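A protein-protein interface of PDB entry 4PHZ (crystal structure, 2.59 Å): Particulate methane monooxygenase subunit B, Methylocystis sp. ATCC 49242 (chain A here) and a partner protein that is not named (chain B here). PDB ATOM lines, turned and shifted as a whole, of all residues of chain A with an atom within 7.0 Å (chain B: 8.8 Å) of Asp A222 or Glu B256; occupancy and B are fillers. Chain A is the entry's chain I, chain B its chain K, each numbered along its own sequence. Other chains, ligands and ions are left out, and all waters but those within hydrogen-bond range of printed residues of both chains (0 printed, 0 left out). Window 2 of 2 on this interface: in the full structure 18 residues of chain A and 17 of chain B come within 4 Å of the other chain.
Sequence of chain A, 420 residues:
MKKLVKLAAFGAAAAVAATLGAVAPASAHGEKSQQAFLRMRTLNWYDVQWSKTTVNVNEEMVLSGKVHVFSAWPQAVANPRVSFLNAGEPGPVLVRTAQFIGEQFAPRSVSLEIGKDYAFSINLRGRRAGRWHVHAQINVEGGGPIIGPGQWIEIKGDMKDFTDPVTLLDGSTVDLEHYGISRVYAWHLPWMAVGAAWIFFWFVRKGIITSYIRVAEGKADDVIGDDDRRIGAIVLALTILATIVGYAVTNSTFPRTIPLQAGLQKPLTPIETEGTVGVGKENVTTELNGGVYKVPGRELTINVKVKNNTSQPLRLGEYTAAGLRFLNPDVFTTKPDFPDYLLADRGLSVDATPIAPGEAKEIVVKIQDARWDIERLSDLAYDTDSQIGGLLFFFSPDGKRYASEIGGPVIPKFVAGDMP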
ATOM      1  N   LYS A 206      20.643   9.237 -15.329  1.00  0.00           N
ATOM      2  CA  LYS A 206      21.986   8.642 -15.481  1.00  0.00           C
ATOM      3  C   LYS A 206      22.883   9.723 -14.948  1.00  0.00           C
ATOM      4  O   LYS A 206      22.524  10.903 -15.006  1.00  0.00           O
ATOM      5  CB  LYS A 206      22.350   8.430 -16.959  1.00  0.00           C
ATOM      6  CG  LYS A 206      21.210   8.129 -17.920  1.00  0.00           C
ATOM      7  CD  LYS A 206      20.806   6.669 -17.797  1.00  0.00           C
ATOM      8  CE  LYS A 206      19.321   6.473 -18.007  1.00  0.00           C
ATOM      9  NZ  LYS A 206      19.089   5.719 -19.257  1.00  0.00           N
ATOM     10  N   THR A 210      28.701   8.526 -13.018  1.00  0.00           N
ATOM     11  CA  THR A 210      28.215   7.151 -13.188  1.00  0.00           C
ATOM     12  C   THR A 210      28.291   6.721 -14.625  1.00  0.00           C
ATOM     13  O   THR A 210      28.776   5.619 -14.919  1.00  0.00           O
ATOM     14  CB  THR A 210      26.753   6.998 -12.759  1.00  0.00           C
ATOM     15  OG1 THR A 210      26.624   7.421 -11.394  1.00  0.00           O
ATOM     16  CG2 THR A 210      26.288   5.553 -12.909  1.00  0.00           C
ATOM     17  N   ILE A 213      31.939   6.430 -16.026  1.00  0.00           N
ATOM     18  CA  ILE A 213      32.420   5.164 -15.461  1.00  0.00           C
ATOM     19  C   ILE A 213      31.818   3.974 -16.200  1.00  0.00           C
ATOM     20  O   ILE A 213      32.561   3.160 -16.748  1.00  0.00           O
ATOM     21  CB  ILE A 213      32.131   5.048 -13.954  1.00  0.00           C
ATOM     22  CG1 ILE A 213      33.079   5.942 -13.143  1.00  0.00           C
ATOM     23  CG2 ILE A 213      32.306   3.620 -13.496  1.00  0.00           C
ATOM     24  CD1 ILE A 213      32.719   6.083 -11.664  1.00  0.00           C
ATOM     25  N   ARG A 214      30.492   3.889 -16.250  1.00  0.00           N
ATOM     26  CA  ARG A 214      29.883   2.746 -16.895  1.00  0.00           C
ATOM     27  C   ARG A 214      30.468   2.550 -18.267  1.00  0.00           C
ATOM     28  O   ARG A 214      30.960   1.454 -18.573  1.00  0.00           O
ATOM     29  CB  ARG A 214      28.381   2.893 -17.014  1.00  0.00           C
ATOM     30  CG  ARG A 214      27.639   2.527 -15.756  1.00  0.00           C
ATOM     31  CD  ARG A 214      26.155   2.547 -15.990  1.00  0.00           C
ATOM     32  NE  ARG A 214      25.470   2.785 -14.728  1.00  0.00           N
ATOM     33  CZ  ARG A 214      24.146   2.795 -14.567  1.00  0.00           C
ATOM     34  NH1 ARG A 214      23.329   2.576 -15.600  1.00  0.00           N
ATOM     35  NH2 ARG A 214      23.635   3.031 -13.363  1.00  0.00           N
ATOM     36  N   VAL A 215      30.428   3.609 -19.080  1.00  0.00           N
ATOM     37  CA  VAL A 215      30.972   3.602 -20.451  1.00  0.00           C
ATOM     38  C   VAL A 215      32.430   3.135 -20.476  1.00  0.00           C
ATOM     39  O   VAL A 215      32.755   2.195 -21.199  1.00  0.00           O
ATOM     40  CB  VAL A 215      30.824   4.987 -21.135  1.00  0.00           C
ATOM     41  CG1 VAL A 215      31.606   5.055 -22.432  1.00  0.00           C
ATOM     42  CG2 VAL A 215      29.363   5.274 -21.391  1.00  0.00           C
ATOM     43  N   GLU A 217      34.103   1.409 -18.196  1.00  0.00           N
ATOM     44  CA  GLU A 217      34.243   0.034 -17.713  1.00  0.00           C
ATOM     45  C   GLU A 217      33.946  -0.976 -18.789  1.00  0.00           C
ATOM     46  O   GLU A 217      34.487  -2.064 -18.754  1.00  0.00           O
ATOM     47  CB  GLU A 217      33.326  -0.256 -16.513  1.00  0.00           C
ATOM     48  CG  GLU A 217      33.689   0.459 -15.211  1.00  0.00           C
ATOM     49  CD  GLU A 217      35.040   0.040 -14.621  1.00  0.00           C
ATOM     50  OE1 GLU A 217      35.062  -0.535 -13.510  1.00  0.00           O
ATOM     51  OE2 GLU A 217      36.093   0.290 -15.247  1.00  0.00           O
ATOM     52  N   GLY A 218      33.083  -0.640 -19.735  1.00  0.00           N
ATOM     53  CA  GLY A 218      32.713  -1.621 -20.729  1.00  0.00           C
ATOM     54  C   GLY A 218      31.283  -1.475 -21.151  1.00  0.00           C
ATOM     55  O   GLY A 218      31.004  -1.575 -22.333  1.00  0.00           O
ATOM     56  N   LYS A 219      30.383  -1.239 -20.195  1.00  0.00           N
ATOM     57  CA  LYS A 219      28.957  -1.030 -20.495  1.00  0.00           C
ATOM     58  C   LYS A 219      28.454   0.261 -19.839  1.00  0.00           C
ATOM     59  O   LYS A 219      28.456   0.340 -18.614  1.00  0.00           O
ATOM     60  CB  LYS A 219      28.115  -2.238 -20.030  1.00  0.00           C
ATOM     61  CG  LYS A 219      28.319  -3.549 -20.797  1.00  0.00           C
ATOM     62  CD  LYS A 219      27.757  -3.503 -22.219  1.00  0.00           C
ATOM     63  CE  LYS A 219      28.858  -3.327 -23.261  1.00  0.00           C
ATOM     64  NZ  LYS A 219      28.416  -2.549 -24.456  1.00  0.00           N
ATOM     65  N   ALA A 220      28.017   1.284 -20.587  1.00  0.00           N
ATOM     66  CA  ALA A 220      27.796   1.381 -22.054  1.00  0.00           C
ATOM     67  C   ALA A 220      26.359   1.068 -22.405  1.00  0.00           C
ATOM     68  O   ALA A 220      25.603   1.971 -22.735  1.00  0.00           O
ATOM     69  CB  ALA A 220      28.777   0.577 -22.889  1.00  0.00           C
ATOM     70  N   ASP A 221      25.968  -0.195 -22.295  1.00  0.00           N
ATOM     71  CA  ASP A 221      24.584  -0.574 -22.556  1.00  0.00           C
ATOM     72  C   ASP A 221      23.775  -0.464 -21.300  1.00  0.00           C
ATOM     73  O   ASP A 221      22.565  -0.634 -21.306  1.00  0.00           O
ATOM     74  CB  ASP A 221      24.493  -1.990 -23.116  1.00  0.00           C
ATOM     75  CG  ASP A 221      24.869  -2.049 -24.575  1.00  0.00           C
ATOM     76  OD1 ASP A 221      24.371  -1.207 -25.355  1.00  0.00           O
ATOM     77  OD2 ASP A 221      25.665  -2.933 -24.945  1.00  0.00           O
ATOM     78  N   ASP A 222      24.463  -0.182 -20.213  1.00  0.00           N
ATOM     79  CA  ASP A 222      23.796   0.033 -18.951  1.00  0.00           C
ATOM     80  C   ASP A 222      23.290   1.461 -18.912  1.00  0.00           C
ATOM     81  O   ASP A 222      22.327   1.772 -18.209  1.00  0.00           O
ATOM     82  CB  ASP A 222      24.760  -0.239 -17.788  1.00  0.00           C
ATOM     83  CG  ASP A 222      25.024  -1.736 -17.571  1.00  0.00           C
ATOM     84  OD1 ASP A 222      25.064  -2.515 -18.560  1.00  0.00           O
ATOM     85  OD2 ASP A 222      25.203  -2.126 -16.394  1.00  0.00           O
ATOM     86  N   VAL A 223      23.951   2.321 -19.683  1.00  0.00           N
ATOM     87  CA  VAL A 223      23.586   3.732 -19.747  1.00  0.00           C
ATOM     88  C   VAL A 223      22.343   3.932 -20.602  1.00  0.00           C
ATOM     89  O   VAL A 223      21.385   4.594 -20.178  1.00  0.00           O
ATOM     90  CB  VAL A 223      24.714   4.611 -20.307  1.00  0.00           C
ATOM     91  CG1 VAL A 223      24.370   6.086 -20.085  1.00  0.00           C
ATOM     92  CG2 VAL A 223      26.041   4.255 -19.650  1.00  0.00           C
ATOM     93  N   ILE A 224      22.382   3.347 -21.797  1.00  0.00           N
ATOM     94  CA  ILE A 224      21.300   3.454 -22.763  1.00  0.00           C
ATOM     95  C   ILE A 224      20.929   2.090 -23.327  1.00  0.00           C
ATOM     96  O   ILE A 224      21.711   1.456 -24.053  1.00  0.00           O
ATOM     97  CB  ILE A 224      21.656   4.415 -23.935  1.00  0.00           C
ATOM     98  CG1 ILE A 224      21.704   5.877 -23.466  1.00  0.00           C
ATOM     99  CG2 ILE A 224      20.666   4.265 -25.077  1.00  0.00           C
ATOM    100  CD1 ILE A 224      20.401   6.427 -22.924  1.00  0.00           C
ATOM    101  N   GLY A 225      19.735   1.638 -22.981  1.00  0.00           N
ATOM    102  CA  GLY A 225      19.078   0.591 -23.751  1.00  0.00           C
ATOM    103  C   GLY A 225      17.702   1.142 -24.038  1.00  0.00           C
ATOM    104  O   GLY A 225      17.272   2.057 -23.333  1.00  0.00           O
ATOM    105  N   ASP A 228      15.116   3.621 -23.227  1.00  0.00           N
ATOM    106  CA  ASP A 228      15.588   5.013 -23.267  1.00  0.00           C
ATOM    107  C   ASP A 228      15.324   5.545 -24.672  1.00  0.00           C
ATOM    108  O   ASP A 228      14.884   6.685 -24.855  1.00  0.00           O
ATOM    109  CB  ASP A 228      17.070   5.099 -22.936  1.00  0.00           C
ATOM    110  CG  ASP A 228      17.374   4.667 -21.518  1.00  0.00           C
ATOM    111  OD1 ASP A 228      16.851   5.309 -20.583  1.00  0.00           O
ATOM    112  OD2 ASP A 228      18.144   3.693 -21.337  1.00  0.00           O
ATOM    113  N   HIS B 243      37.907   8.180 -11.587  1.00  0.00           N
ATOM    114  CA  HIS B 243      37.642   6.738 -11.797  1.00  0.00           C
ATOM    115  C   HIS B 243      38.624   5.883 -11.069  1.00  0.00           C
ATOM    116  O   HIS B 243      38.237   4.913 -10.409  1.00  0.00           O
ATOM    117  CB  HIS B 243      37.732   6.412 -13.279  1.00  0.00           C
ATOM    118  CG  HIS B 243      37.268   5.013 -13.648  1.00  0.00           C
ATOM    119  ND1 HIS B 243      37.541   4.454 -14.853  1.00  0.00           N
ATOM    120  CD2 HIS B 243      36.511   4.072 -12.944  1.00  0.00           C
ATOM    121  CE1 HIS B 243      36.979   3.230 -14.914  1.00  0.00           C
ATOM    122  NE2 HIS B 243      36.361   2.993 -13.747  1.00  0.00           N
ATOM    123  N   VAL B 246      38.496   6.134  -7.016  1.00  0.00           N
ATOM    124  CA  VAL B 246      37.427   5.339  -6.463  1.00  0.00           C
ATOM    125  C   VAL B 246      37.840   3.860  -6.602  1.00  0.00           C
ATOM    126  O   VAL B 246      38.276   3.406  -7.666  1.00  0.00           O
ATOM    127  CB  VAL B 246      36.097   5.664  -7.181  1.00  0.00           C
ATOM    128  CG1 VAL B 246      34.976   4.765  -6.686  1.00  0.00           C
ATOM    129  CG2 VAL B 246      35.740   7.121  -6.948  1.00  0.00           C
ATOM    130  N   LYS B 248      37.781  -0.327  -6.815  1.00  0.00           N
ATOM    131  CA  LYS B 248      36.962  -1.290  -7.555  1.00  0.00           C
ATOM    132  C   LYS B 248      35.584  -1.413  -6.875  1.00  0.00           C
ATOM    133  O   LYS B 248      34.598  -1.848  -7.483  1.00  0.00           O
ATOM    134  CB  LYS B 248      37.705  -2.636  -7.625  1.00  0.00           C
ATOM    135  CG  LYS B 248      36.908  -3.837  -8.126  1.00  0.00           C
ATOM    136  CD  LYS B 248      36.291  -4.644  -6.987  1.00  0.00           C
ATOM    137  CE  LYS B 248      34.998  -5.335  -7.415  1.00  0.00           C
ATOM    138  NZ  LYS B 248      34.149  -5.691  -6.241  1.00  0.00           N
ATOM    139  N   GLU B 249      35.530  -0.986  -5.615  1.00  0.00           N
ATOM    140  CA  GLU B 249      34.336  -1.106  -4.791  1.00  0.00           C
ATOM    141  C   GLU B 249      33.385   0.058  -4.997  1.00  0.00           C
ATOM    142  O   GLU B 249      32.250  -0.149  -5.441  1.00  0.00           O
ATOM    143  CB  GLU B 249      34.709  -1.273  -3.319  1.00  0.00           C
ATOM    144  CG  GLU B 249      35.191  -2.684  -2.982  1.00  0.00           C
ATOM    145  CD  GLU B 249      36.100  -2.736  -1.761  1.00  0.00           C
ATOM    146  OE1 GLU B 249      36.886  -1.787  -1.542  1.00  0.00           O
ATOM    147  OE2 GLU B 249      36.044  -3.735  -1.014  1.00  0.00           O
ATOM    148  N   GLY B 250      33.844   1.274  -4.698  1.00  0.00           N
ATOM    149  CA  GLY B 250      33.103   2.474  -5.073  1.00  0.00           C
ATOM    150  C   GLY B 250      32.615   2.409  -6.518  1.00  0.00           C
ATOM    151  O   GLY B 250      31.458   2.706  -6.813  1.00  0.00           O
ATOM    152  N   VAL B 251      33.503   1.992  -7.413  1.00  0.00           N
ATOM    153  CA  VAL B 251      33.212   1.882  -8.843  1.00  0.00           C
ATOM    154  C   VAL B 251      32.144   0.825  -9.121  1.00  0.00           C
ATOM    155  O   VAL B 251      30.965   1.031  -8.819  1.00  0.00           O
ATOM    156  CB  VAL B 251      34.506   1.612  -9.663  1.00  0.00           C
ATOM    157  CG1 VAL B 251      34.210   1.164 -11.079  1.00  0.00           C
ATOM    158  CG2 VAL B 251      35.383   2.849  -9.698  1.00  0.00           C
ATOM    159  N   LYS B 252      32.584  -0.303  -9.680  1.00  0.00           N
ATOM    160  CA  LYS B 252      31.724  -1.382 -10.179  1.00  0.00           C
ATOM    161  C   LYS B 252      30.535  -1.638  -9.271  1.00  0.00           C
ATOM    162  O   LYS B 252      29.401  -1.779  -9.747  1.00  0.00           O
ATOM    163  CB  LYS B 252      32.529  -2.682 -10.363  1.00  0.00           C
ATOM    164  CG  LYS B 252      33.574  -2.632 -11.470  1.00  0.00           C
ATOM    165  CD  LYS B 252      34.789  -3.485 -11.134  1.00  0.00           C
ATOM    166  CE  LYS B 252      36.068  -2.801 -11.594  1.00  0.00           C
ATOM    167  NZ  LYS B 252      37.286  -3.611 -11.324  1.00  0.00           N
ATOM    168  N   LEU B 253      30.797  -1.681  -7.967  1.00  0.00           N
ATOM    169  CA  LEU B 253      29.744  -1.958  -7.011  1.00  0.00           C
ATOM    170  C   LEU B 253      28.865  -0.731  -6.733  1.00  0.00           C
ATOM    171  O   LEU B 253      27.713  -0.681  -7.175  1.00  0.00           O
ATOM    172  CB  LEU B 253      30.312  -2.569  -5.712  1.00  0.00           C
ATOM    173  CG  LEU B 253      30.989  -3.957  -5.718  1.00  0.00           C
ATOM    174  CD1 LEU B 253      31.687  -4.235  -4.388  1.00  0.00           C
ATOM    175  CD2 LEU B 253      30.012  -5.081  -6.057  1.00  0.00           C
ATOM    176  N   LEU B 254      29.411   0.264  -6.045  1.00  0.00           N
ATOM    177  CA  LEU B 254      28.565   1.251  -5.364  1.00  0.00           C
ATOM    178  C   LEU B 254      27.764   2.173  -6.261  1.00  0.00           C
ATOM    179  O   LEU B 254      26.553   2.302  -6.095  1.00  0.00           O
ATOM    180  CB  LEU B 254      29.355   2.045  -4.311  1.00  0.00           C
ATOM    181  CG  LEU B 254      29.439   1.450  -2.892  1.00  0.00           C
ATOM    182  CD1 LEU B 254      28.073   1.437  -2.207  1.00  0.00           C
ATOM    183  CD2 LEU B 254      30.072   0.056  -2.868  1.00  0.00           C
ATOM    184  N   THR B 255      28.431   2.816  -7.210  1.00  0.00           N
ATOM    185  CA  THR B 255      27.734   3.644  -8.191  1.00  0.00           C
ATOM    186  C   THR B 255      27.175   2.772  -9.335  1.00  0.00           C
ATOM    187  O   THR B 255      26.425   3.255 -10.189  1.00  0.00           O
ATOM    188  CB  THR B 255      28.641   4.772  -8.739  1.00  0.00           C
ATOM    189  OG1 THR B 255      29.811   4.196  -9.325  1.00  0.00           O
ATOM    190  CG2 THR B 255      29.057   5.748  -7.631  1.00  0.00           C
ATOM    191  N   GLU B 256      27.535   1.486  -9.317  1.00  0.00           N
ATOM    192  CA  GLU B 256      27.035   0.468 -10.254  1.00  0.00           C
ATOM    193  C   GLU B 256      27.642   0.660 -11.632  1.00  0.00           C
ATOM    194  O   GLU B 256      28.795   1.063 -11.746  1.00  0.00           O
ATOM    195  CB  GLU B 256      25.498   0.448 -10.301  1.00  0.00           C
ATOM    196  CG  GLU B 256      24.883  -0.877 -10.735  1.00  0.00           C
ATOM    197  CD  GLU B 256      24.693  -0.999 -12.244  1.00  0.00           C
ATOM    198  OE1 GLU B 256      25.033  -0.054 -12.990  1.00  0.00           O
ATOM    199  OE2 GLU B 256      24.189  -2.048 -12.697  1.00  0.00           O
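NE of Arg A214 lies within salt-bridge range of OE1 of Glu B256.
OE2 of Glu A217 lies close to NE2 of His B243, 3.1 Å away.
The backbone carbonyl oxygen (O) of Gly B250 lies within hydrogen-bond range of the backbone NH (N) of Thr B255 (3.1 Å).
The backbone carbonyl oxygen (O) of Val B251 is in hydrogen-bond range of the side-chain hydroxyl (OG1) of Thr B255 (3.4 Å).
The backbone NH of Glu B256 lies within hydrogen-bond range of the backbone carbonyl oxygen of Val B251 (3.5 Å).
The guanidinium group (NH1) of Arg A214 lies within hydrogen-bond range of the backbone carbonyl oxygen (O) of Asp A222, 2.9 Å away.
The backbone carbonyl oxygen (O) of Arg A214 lies close to the backbone NH (N) of Lys A219, at 3.2 Å.
Among the printed residues, pairs that only touch across the chains: Glu A217 with Val B251, Glu A217 with Lys B252, Thr A210 with Thr B255, Asp A222 with Glu B256, Ile A213 with His B243 and Ile A213 with Val B251.
Asp A222 touches just one residue of chain B: Glu B256.
Of the printed residues of chain A, Thr B255 touches Thr A210.
Printed residues of chain A within 4 Å of His B243: Ile A213 and Glu A217.
Printed residues of chain B within 4 Å of Thr A210: Thr B255 (3.6 Å).
Of the printed residues of chain B, Ile A213 touches His B243 and Val B251.
Of the printed residues of chain B, Glu A217 touches His B243, Val B251 and Lys B252.
Leu B254 touches none of the printed residues of chain A.
Hydrophobic or aromatic side chains of chain B that line the printed part of chain A: His B243 and Val B251.
Among the printed residues, 8 pairs touch across the chains.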
